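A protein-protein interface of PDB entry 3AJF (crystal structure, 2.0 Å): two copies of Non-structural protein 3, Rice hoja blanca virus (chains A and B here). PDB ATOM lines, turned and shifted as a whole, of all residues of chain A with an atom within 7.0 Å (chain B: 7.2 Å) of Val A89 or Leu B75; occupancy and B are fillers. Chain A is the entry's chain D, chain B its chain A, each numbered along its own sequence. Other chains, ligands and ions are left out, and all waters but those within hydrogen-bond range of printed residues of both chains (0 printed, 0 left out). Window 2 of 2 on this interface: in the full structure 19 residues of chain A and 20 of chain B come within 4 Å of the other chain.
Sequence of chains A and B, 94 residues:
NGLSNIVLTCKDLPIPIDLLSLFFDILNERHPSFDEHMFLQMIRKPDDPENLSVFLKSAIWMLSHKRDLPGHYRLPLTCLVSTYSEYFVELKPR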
ATOM      1  N   SER A  85     -24.558  13.452   2.744  1.00  0.00           N
ATOM      2  CA  SER A  85     -24.732  12.626   3.941  1.00  0.00           C
ATOM      3  C   SER A  85     -26.156  12.720   4.523  1.00  0.00           C
ATOM      4  O   SER A  85     -26.638  11.772   5.123  1.00  0.00           O
ATOM      5  CB  SER A  85     -23.625  12.906   4.975  1.00  0.00           C
ATOM      6  OG  SER A  85     -24.021  14.046   5.722  1.00  0.00           O
ATOM      7  N   GLU A  86     -26.847  13.836   4.304  1.00  0.00           N
ATOM      8  CA  GLU A  86     -28.224  14.029   4.802  1.00  0.00           C
ATOM      9  C   GLU A  86     -29.235  12.971   4.315  1.00  0.00           C
ATOM     10  O   GLU A  86     -30.206  12.669   4.993  1.00  0.00           O
ATOM     11  CB  GLU A  86     -28.776  15.412   4.403  1.00  0.00           C
ATOM     12  CG  GLU A  86     -28.107  16.648   5.052  1.00  0.00           C
ATOM     13  CD  GLU A  86     -28.797  18.006   4.670  1.00  0.00           C
ATOM     14  OE1 GLU A  86     -30.041  18.094   4.625  1.00  0.00           O
ATOM     15  OE2 GLU A  86     -28.070  18.983   4.389  1.00  0.00           O
ATOM     16  N   TYR A  87     -28.994  12.400   3.133  1.00  0.00           N
ATOM     17  CA  TYR A  87     -29.915  11.375   2.582  1.00  0.00           C
ATOM     18  C   TYR A  87     -29.969  10.115   3.438  1.00  0.00           C
ATOM     19  O   TYR A  87     -30.895   9.320   3.270  1.00  0.00           O
ATOM     20  CB  TYR A  87     -29.500  11.015   1.136  1.00  0.00           C
ATOM     21  CG  TYR A  87     -29.867  12.118   0.176  1.00  0.00           C
ATOM     22  CD1 TYR A  87     -31.160  12.207  -0.344  1.00  0.00           C
ATOM     23  CD2 TYR A  87     -28.929  13.095  -0.182  1.00  0.00           C
ATOM     24  CE1 TYR A  87     -31.510  13.264  -1.242  1.00  0.00           C
ATOM     25  CE2 TYR A  87     -29.274  14.145  -1.044  1.00  0.00           C
ATOM     26  CZ  TYR A  87     -30.542  14.213  -1.581  1.00  0.00           C
ATOM     27  OH  TYR A  87     -30.849  15.265  -2.431  1.00  0.00           O
ATOM     28  N   PHE A  88     -28.993   9.930   4.353  1.00  0.00           N
ATOM     29  CA  PHE A  88     -29.034   8.766   5.252  1.00  0.00           C
ATOM     30  C   PHE A  88     -30.200   8.794   6.242  1.00  0.00           C
ATOM     31  O   PHE A  88     -30.536   7.763   6.822  1.00  0.00           O
ATOM     32  CB  PHE A  88     -27.727   8.542   6.049  1.00  0.00           C
ATOM     33  CG  PHE A  88     -26.638   7.844   5.265  1.00  0.00           C
ATOM     34  CD1 PHE A  88     -26.867   6.607   4.664  1.00  0.00           C
ATOM     35  CD2 PHE A  88     -25.386   8.415   5.144  1.00  0.00           C
ATOM     36  CE1 PHE A  88     -25.869   5.956   3.955  1.00  0.00           C
ATOM     37  CE2 PHE A  88     -24.368   7.758   4.412  1.00  0.00           C
ATOM     38  CZ  PHE A  88     -24.618   6.530   3.825  1.00  0.00           C
ATOM     39  N   VAL A  89     -30.813   9.954   6.478  1.00  0.00           N
ATOM     40  CA  VAL A  89     -31.928   9.956   7.451  1.00  0.00           C
ATOM     41  C   VAL A  89     -32.999   8.961   7.002  1.00  0.00           C
ATOM     42  O   VAL A  89     -33.415   8.105   7.791  1.00  0.00           O
ATOM     43  CB  VAL A  89     -32.545  11.348   7.699  1.00  0.00           C
ATOM     44  CG1 VAL A  89     -33.682  11.253   8.732  1.00  0.00           C
ATOM     45  CG2 VAL A  89     -31.462  12.352   8.163  1.00  0.00           C
ATOM     46  N   GLU A  90     -33.417   9.035   5.739  1.00  0.00           N
ATOM     47  CA  GLU A  90     -34.442   8.099   5.225  1.00  0.00           C
ATOM     48  C   GLU A  90     -33.872   6.880   4.508  1.00  0.00           C
ATOM     49  O   GLU A  90     -34.537   5.876   4.402  1.00  0.00           O
ATOM     50  CB  GLU A  90     -35.440   8.786   4.278  1.00  0.00           C
ATOM     51  CG  GLU A  90     -35.926  10.187   4.674  1.00  0.00           C
ATOM     52  CD  GLU A  90     -36.881  10.208   5.832  1.00  0.00           C
ATOM     53  OE1 GLU A  90     -36.981   9.186   6.552  1.00  0.00           O
ATOM     54  OE2 GLU A  90     -37.549  11.260   6.023  1.00  0.00           O
ATOM     55  N   LEU A  91     -32.662   6.972   3.985  1.00  0.00           N
ATOM     56  CA  LEU A  91     -32.078   5.868   3.225  1.00  0.00           C
ATOM     57  C   LEU A  91     -31.384   4.848   4.151  1.00  0.00           C
ATOM     58  O   LEU A  91     -30.246   5.054   4.584  1.00  0.00           O
ATOM     59  CB  LEU A  91     -31.135   6.435   2.159  1.00  0.00           C
ATOM     60  CG  LEU A  91     -30.540   5.567   1.069  1.00  0.00           C
ATOM     61  CD1 LEU A  91     -31.616   5.136   0.058  1.00  0.00           C
ATOM     62  CD2 LEU A  91     -29.416   6.375   0.393  1.00  0.00           C
ATOM     63  N   LYS A  92     -32.100   3.772   4.468  1.00  0.00           N
ATOM     64  CA  LYS A  92     -31.704   2.775   5.488  1.00  0.00           C
ATOM     65  C   LYS A  92     -31.236   1.471   4.833  1.00  0.00           C
ATOM     66  O   LYS A  92     -31.687   1.164   3.734  1.00  0.00           O
ATOM     67  CB  LYS A  92     -32.924   2.368   6.327  1.00  0.00           C
ATOM     68  CG  LYS A  92     -33.729   3.475   6.966  1.00  0.00           C
ATOM     69  CD  LYS A  92     -34.806   2.851   7.786  1.00  0.00           C
ATOM     70  CE  LYS A  92     -35.898   3.826   8.159  1.00  0.00           C
ATOM     71  NZ  LYS A  92     -37.112   3.089   8.689  1.00  0.00           N
ATOM     72  N   CYS B  10     -27.128  19.080  18.210  1.00  0.00           N
ATOM     73  CA  CYS B  10     -26.327  19.267  17.009  1.00  0.00           C
ATOM     74  C   CYS B  10     -27.231  20.047  16.074  1.00  0.00           C
ATOM     75  O   CYS B  10     -28.290  19.554  15.717  1.00  0.00           O
ATOM     76  CB  CYS B  10     -26.018  17.894  16.384  1.00  0.00           C
ATOM     77  SG  CYS B  10     -25.340  17.931  14.674  1.00  0.00           S
ATOM     78  N   LEU B  13     -30.789  20.031  17.007  1.00  0.00           N
ATOM     79  CA  LEU B  13     -31.445  18.735  17.067  1.00  0.00           C
ATOM     80  C   LEU B  13     -30.837  17.956  18.228  1.00  0.00           C
ATOM     81  O   LEU B  13     -29.608  17.836  18.305  1.00  0.00           O
ATOM     82  CB  LEU B  13     -31.209  17.950  15.767  1.00  0.00           C
ATOM     83  CG  LEU B  13     -31.529  18.558  14.393  1.00  0.00           C
ATOM     84  CD1 LEU B  13     -31.001  17.655  13.251  1.00  0.00           C
ATOM     85  CD2 LEU B  13     -33.020  18.824  14.207  1.00  0.00           C
ATOM     86  N   PRO B  14     -31.682  17.431  19.126  1.00  0.00           N
ATOM     87  CA  PRO B  14     -31.249  16.620  20.263  1.00  0.00           C
ATOM     88  C   PRO B  14     -30.495  15.354  19.849  1.00  0.00           C
ATOM     89  O   PRO B  14     -30.938  14.614  18.965  1.00  0.00           O
ATOM     90  CB  PRO B  14     -32.558  16.245  20.947  1.00  0.00           C
ATOM     91  CG  PRO B  14     -33.510  17.370  20.565  1.00  0.00           C
ATOM     92  CD  PRO B  14     -33.143  17.647  19.135  1.00  0.00           C
ATOM     93  N   LEU B  19     -26.612   7.444  22.099  1.00  0.00           N
ATOM     94  CA  LEU B  19     -26.109   7.423  20.726  1.00  0.00           C
ATOM     95  C   LEU B  19     -24.616   7.717  20.711  1.00  0.00           C
ATOM     96  O   LEU B  19     -23.852   7.046  20.011  1.00  0.00           O
ATOM     97  CB  LEU B  19     -26.860   8.404  19.800  1.00  0.00           C
ATOM     98  CG  LEU B  19     -26.252   8.599  18.382  1.00  0.00           C
ATOM     99  CD1 LEU B  19     -26.061   7.256  17.590  1.00  0.00           C
ATOM    100  CD2 LEU B  19     -27.080   9.526  17.561  1.00  0.00           C
ATOM    101  N   LEU B  63     -24.822   4.033   9.637  1.00  0.00           N
ATOM    102  CA  LEU B  63     -25.993   4.468   8.866  1.00  0.00           C
ATOM    103  C   LEU B  63     -26.233   3.616   7.615  1.00  0.00           C
ATOM    104  O   LEU B  63     -27.376   3.467   7.162  1.00  0.00           O
ATOM    105  CB  LEU B  63     -25.842   5.937   8.450  1.00  0.00           C
ATOM    106  CG  LEU B  63     -25.920   6.946   9.595  1.00  0.00           C
ATOM    107  CD1 LEU B  63     -25.314   8.329   9.216  1.00  0.00           C
ATOM    108  CD2 LEU B  63     -27.389   7.058  10.023  1.00  0.00           C
ATOM    109  N   LEU B  69     -29.735  -0.251  14.000  1.00  0.00           N
ATOM    110  CA  LEU B  69     -29.579   1.102  14.554  1.00  0.00           C
ATOM    111  C   LEU B  69     -30.987   1.586  14.908  1.00  0.00           C
ATOM    112  O   LEU B  69     -31.869   1.540  14.054  1.00  0.00           O
ATOM    113  CB  LEU B  69     -28.933   2.037  13.523  1.00  0.00           C
ATOM    114  CG  LEU B  69     -28.594   3.461  13.975  1.00  0.00           C
ATOM    115  CD1 LEU B  69     -27.402   3.429  14.949  1.00  0.00           C
ATOM    116  CD2 LEU B  69     -28.329   4.390  12.774  1.00  0.00           C
ATOM    117  N   PRO B  70     -31.229   1.999  16.167  1.00  0.00           N
ATOM    118  CA  PRO B  70     -32.581   2.508  16.443  1.00  0.00           C
ATOM    119  C   PRO B  70     -33.043   3.620  15.463  1.00  0.00           C
ATOM    120  O   PRO B  70     -32.253   4.476  15.050  1.00  0.00           O
ATOM    121  CB  PRO B  70     -32.456   3.049  17.868  1.00  0.00           C
ATOM    122  CG  PRO B  70     -31.390   2.215  18.494  1.00  0.00           C
ATOM    123  CD  PRO B  70     -30.379   2.007  17.373  1.00  0.00           C
ATOM    124  N   GLY B  71     -34.310   3.577  15.063  1.00  0.00           N
ATOM    125  CA  GLY B  71     -34.860   4.536  14.102  1.00  0.00           C
ATOM    126  C   GLY B  71     -34.661   5.993  14.513  1.00  0.00           C
ATOM    127  O   GLY B  71     -34.337   6.840  13.690  1.00  0.00           O
ATOM    128  N   HIS B  72     -34.829   6.288  15.794  1.00  0.00           N
ATOM    129  CA  HIS B  72     -34.689   7.666  16.262  1.00  0.00           C
ATOM    130  C   HIS B  72     -33.237   8.140  16.356  1.00  0.00           C
ATOM    131  O   HIS B  72     -32.987   9.289  16.659  1.00  0.00           O
ATOM    132  CB  HIS B  72     -35.461   7.900  17.568  1.00  0.00           C
ATOM    133  CG  HIS B  72     -34.896   7.184  18.756  1.00  0.00           C
ATOM    134  ND1 HIS B  72     -34.924   5.811  18.882  1.00  0.00           N
ATOM    135  CD2 HIS B  72     -34.319   7.655  19.889  1.00  0.00           C
ATOM    136  CE1 HIS B  72     -34.358   5.464  20.024  1.00  0.00           C
ATOM    137  NE2 HIS B  72     -33.992   6.564  20.658  1.00  0.00           N
ATOM    138  N   TYR B  73     -32.289   7.250  16.080  1.00  0.00           N
ATOM    139  CA  TYR B  73     -30.888   7.623  16.056  1.00  0.00           C
ATOM    140  C   TYR B  73     -30.483   8.142  14.685  1.00  0.00           C
ATOM    141  O   TYR B  73     -29.445   8.782  14.571  1.00  0.00           O
ATOM    142  CB  TYR B  73     -29.994   6.436  16.464  1.00  0.00           C
ATOM    143  CG  TYR B  73     -29.927   6.142  17.967  1.00  0.00           C
ATOM    144  CD1 TYR B  73     -30.819   6.739  18.882  1.00  0.00           C
ATOM    145  CD2 TYR B  73     -28.981   5.252  18.464  1.00  0.00           C
ATOM    146  CE1 TYR B  73     -30.735   6.477  20.247  1.00  0.00           C
ATOM    147  CE2 TYR B  73     -28.903   4.977  19.827  1.00  0.00           C
ATOM    148  CZ  TYR B  73     -29.778   5.591  20.697  1.00  0.00           C
ATOM    149  OH  TYR B  73     -29.686   5.299  22.024  1.00  0.00           O
ATOM    150  N   ARG B  74     -31.310   7.914  13.652  1.00  0.00           N
ATOM    151  CA  ARG B  74     -30.843   8.224  12.293  1.00  0.00           C
ATOM    152  C   ARG B  74     -30.583   9.711  12.049  1.00  0.00           C
ATOM    153  O   ARG B  74     -29.573  10.074  11.426  1.00  0.00           O
ATOM    154  CB  ARG B  74     -31.753   7.636  11.189  1.00  0.00           C
ATOM    155  CG  ARG B  74     -31.907   6.102  11.220  1.00  0.00           C
ATOM    156  CD  ARG B  74     -32.478   5.591   9.899  1.00  0.00           C
ATOM    157  NE  ARG B  74     -31.461   5.677   8.853  1.00  0.00           N
ATOM    158  CZ  ARG B  74     -30.440   4.838   8.706  1.00  0.00           C
ATOM    159  NH1 ARG B  74     -30.326   3.772   9.482  1.00  0.00           N
ATOM    160  NH2 ARG B  74     -29.552   5.034   7.737  1.00  0.00           N
ATOM    161  N   LEU B  75     -31.494  10.550  12.518  1.00  0.00           N
ATOM    162  CA  LEU B  75     -31.405  11.992  12.263  1.00  0.00           C
ATOM    163  C   LEU B  75     -30.239  12.635  13.039  1.00  0.00           C
ATOM    164  O   LEU B  75     -29.431  13.366  12.444  1.00  0.00           O
ATOM    165  CB  LEU B  75     -32.746  12.692  12.549  1.00  0.00           C
ATOM    166  CG  LEU B  75     -32.821  14.215  12.352  1.00  0.00           C
ATOM    167  CD1 LEU B  75     -32.299  14.616  10.968  1.00  0.00           C
ATOM    168  CD2 LEU B  75     -34.239  14.733  12.560  1.00  0.00           C
ATOM    169  N   PRO B  76     -30.146  12.370  14.354  1.00  0.00           N
ATOM    170  CA  PRO B  76     -28.986  12.910  15.077  1.00  0.00           C
ATOM    171  C   PRO B  76     -27.628  12.392  14.581  1.00  0.00           C
ATOM    172  O   PRO B  76     -26.665  13.163  14.555  1.00  0.00           O
ATOM    173  CB  PRO B  76     -29.220  12.507  16.529  1.00  0.00           C
ATOM    174  CG  PRO B  76     -30.433  11.593  16.548  1.00  0.00           C
ATOM    175  CD  PRO B  76     -31.122  11.690  15.236  1.00  0.00           C
ATOM    176  N   LEU B  77     -27.549  11.125  14.178  1.00  0.00           N
ATOM    177  CA  LEU B  77     -26.277  10.585  13.753  1.00  0.00           C
ATOM    178  C   LEU B  77     -25.881  11.188  12.405  1.00  0.00           C
ATOM    179  O   LEU B  77     -24.717  11.510  12.178  1.00  0.00           O
ATOM    180  CB  LEU B  77     -26.327   9.054  13.695  1.00  0.00           C
ATOM    181  CG  LEU B  77     -25.049   8.303  13.313  1.00  0.00           C
ATOM    182  CD1 LEU B  77     -23.870   8.743  14.198  1.00  0.00           C
ATOM    183  CD2 LEU B  77     -25.294   6.797  13.417  1.00  0.00           C
ATOM    184  N   THR B  78     -26.863  11.377  11.528  1.00  0.00           N
ATOM    185  CA  THR B  78     -26.613  12.015  10.264  1.00  0.00           C
ATOM    186  C   THR B  78     -26.188  13.460  10.494  1.00  0.00           C
ATOM    187  O   THR B  78     -25.303  13.971   9.786  1.00  0.00           O
ATOM    188  CB  THR B  78     -27.887  11.963   9.380  1.00  0.00           C
ATOM    189  OG1 THR B  78     -28.175  10.594   9.067  1.00  0.00           O
ATOM    190  CG2 THR B  78     -27.695  12.734   8.101  1.00  0.00           C
ATOM    191  N   CYS B  79     -26.818  14.119  11.463  1.00  0.00           N
ATOM    192  CA  CYS B  79     -26.418  15.478  11.847  1.00  0.00           C
ATOM    193  C   CYS B  79     -24.934  15.514  12.207  1.00  0.00           C
ATOM    194  O   CYS B  79     -24.197  16.392  11.740  1.00  0.00           O
ATOM    195  CB  CYS B  79     -27.241  16.024  13.050  1.00  0.00           C
ATOM    196  SG  CYS B  79     -26.960  17.806  13.364  1.00  0.00           S
ATOM    197  N   LEU B  80     -24.506  14.571  13.051  1.00  0.00           N
ATOM    198  CA  LEU B  80     -23.100  14.487  13.473  1.00  0.00           C
ATOM    199  C   LEU B  80     -22.161  14.313  12.259  1.00  0.00           C
ATOM    200  O   LEU B  80     -21.128  15.012  12.133  1.00  0.00           O
ATOM    201  CB  LEU B  80     -22.930  13.317  14.454  1.00  0.00           C
ATOM    202  CG  LEU B  80     -23.654  13.450  15.802  1.00  0.00           C
ATOM    203  CD1 LEU B  80     -23.427  12.189  16.682  1.00  0.00           C
ATOM    204  CD2 LEU B  80     -23.188  14.738  16.515  1.00  0.00           C
ATOM    205  N   VAL B  81     -22.537  13.414  11.344  1.00  0.00           N
ATOM    206  CA  VAL B  81     -21.739  13.211  10.148  1.00  0.00           C
ATOM    207  C   VAL B  81     -21.625  14.526   9.369  1.00  0.00           C
ATOM    208  O   VAL B  81     -20.525  14.951   8.971  1.00  0.00           O
ATOM    209  CB  VAL B  81     -22.272  12.066   9.232  1.00  0.00           C
ATOM    210  CG1 VAL B  81     -21.548  12.102   7.873  1.00  0.00           C
ATOM    211  CG2 VAL B  81     -22.004  10.782   9.850  1.00  0.00           C
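SG of Cys B10 is disulfide-bonded to SG of Cys B79, 2.1 Å away.
NH2 of Arg B74 sits at hydrogen-bond distance from O of Leu B63, 2.7 Å away.
The side-chain hydroxyl (OG1) of Thr B78 lies within hydrogen-bond range of the backbone carbonyl oxygen (O) of Arg B74 (2.8 Å).
O of Ser A85 touches CG2 of Thr B78, 3.3 Å away.
CB of Ser A85 touches CG1 of Val B81 (3.7 Å).
CA of Glu A86 touches CG2 of Thr B78 (3.6 Å).
Phe A88 touches Leu B63 (CG to CB, 3.8 Å).
Thr B78 touches Phe A88 (OG1 to CB, 3.7 Å).
Leu B75 touches Val A89.
Val A89 touches Thr B78.
Lys A92 touches Arg B74.
Val A89 touches just these residues of chain B: Arg B74, Leu B75 and Thr B78.
Leu B75 touches just one residue of chain A: Val A89 (3.7 Å).
Of the printed residues of chain A, Val B81 touches Ser A85.
Of the printed residues of chain B, Ser A85 touches Thr B78 and Val B81.
Printed residues of chain B within 4 Å of Phe A88: Leu B63 (3.8 Å), Arg B74 (3.0 Å) and Thr B78 (3.7 Å).
Pro B76 touches none of the printed residues of chain A.
The nearest residue of chain A that does not touch Leu B75 is Phe A88 (6.4 Å).
The guanidinium group (NH2) of Arg B74 lies within hydrogen-bond range of the backbone carbonyl oxygen (O) of Leu A91, at 3.2 Å.
The backbone carbonyl oxygen (O) of Phe A88 is in hydrogen-bond range of the guanidinium group (NH2) of Arg B74, 3.0 Å away.
The backbone carbonyl oxygen (O) of Val A89 is in hydrogen-bond range of the guanidinium group (NE) of Arg B74.
Hydrophobic or aromatic side chains of chain B that line the printed part of chain A: Leu B63, Leu B75 and Val B81.
Of the 8 printed residues of chain A, 6 touch a printed residue of chain B.
Hydrophobic or aromatic side chains of chain A within 4 Å of the printed part of chain B: Phe A88 and Val A89.
Among the printed residues, no Asp or Glu carboxylate lies within 4 Å of a Lys or Arg side-chain nitrogen of the other chain.
No position is printed for both chains.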
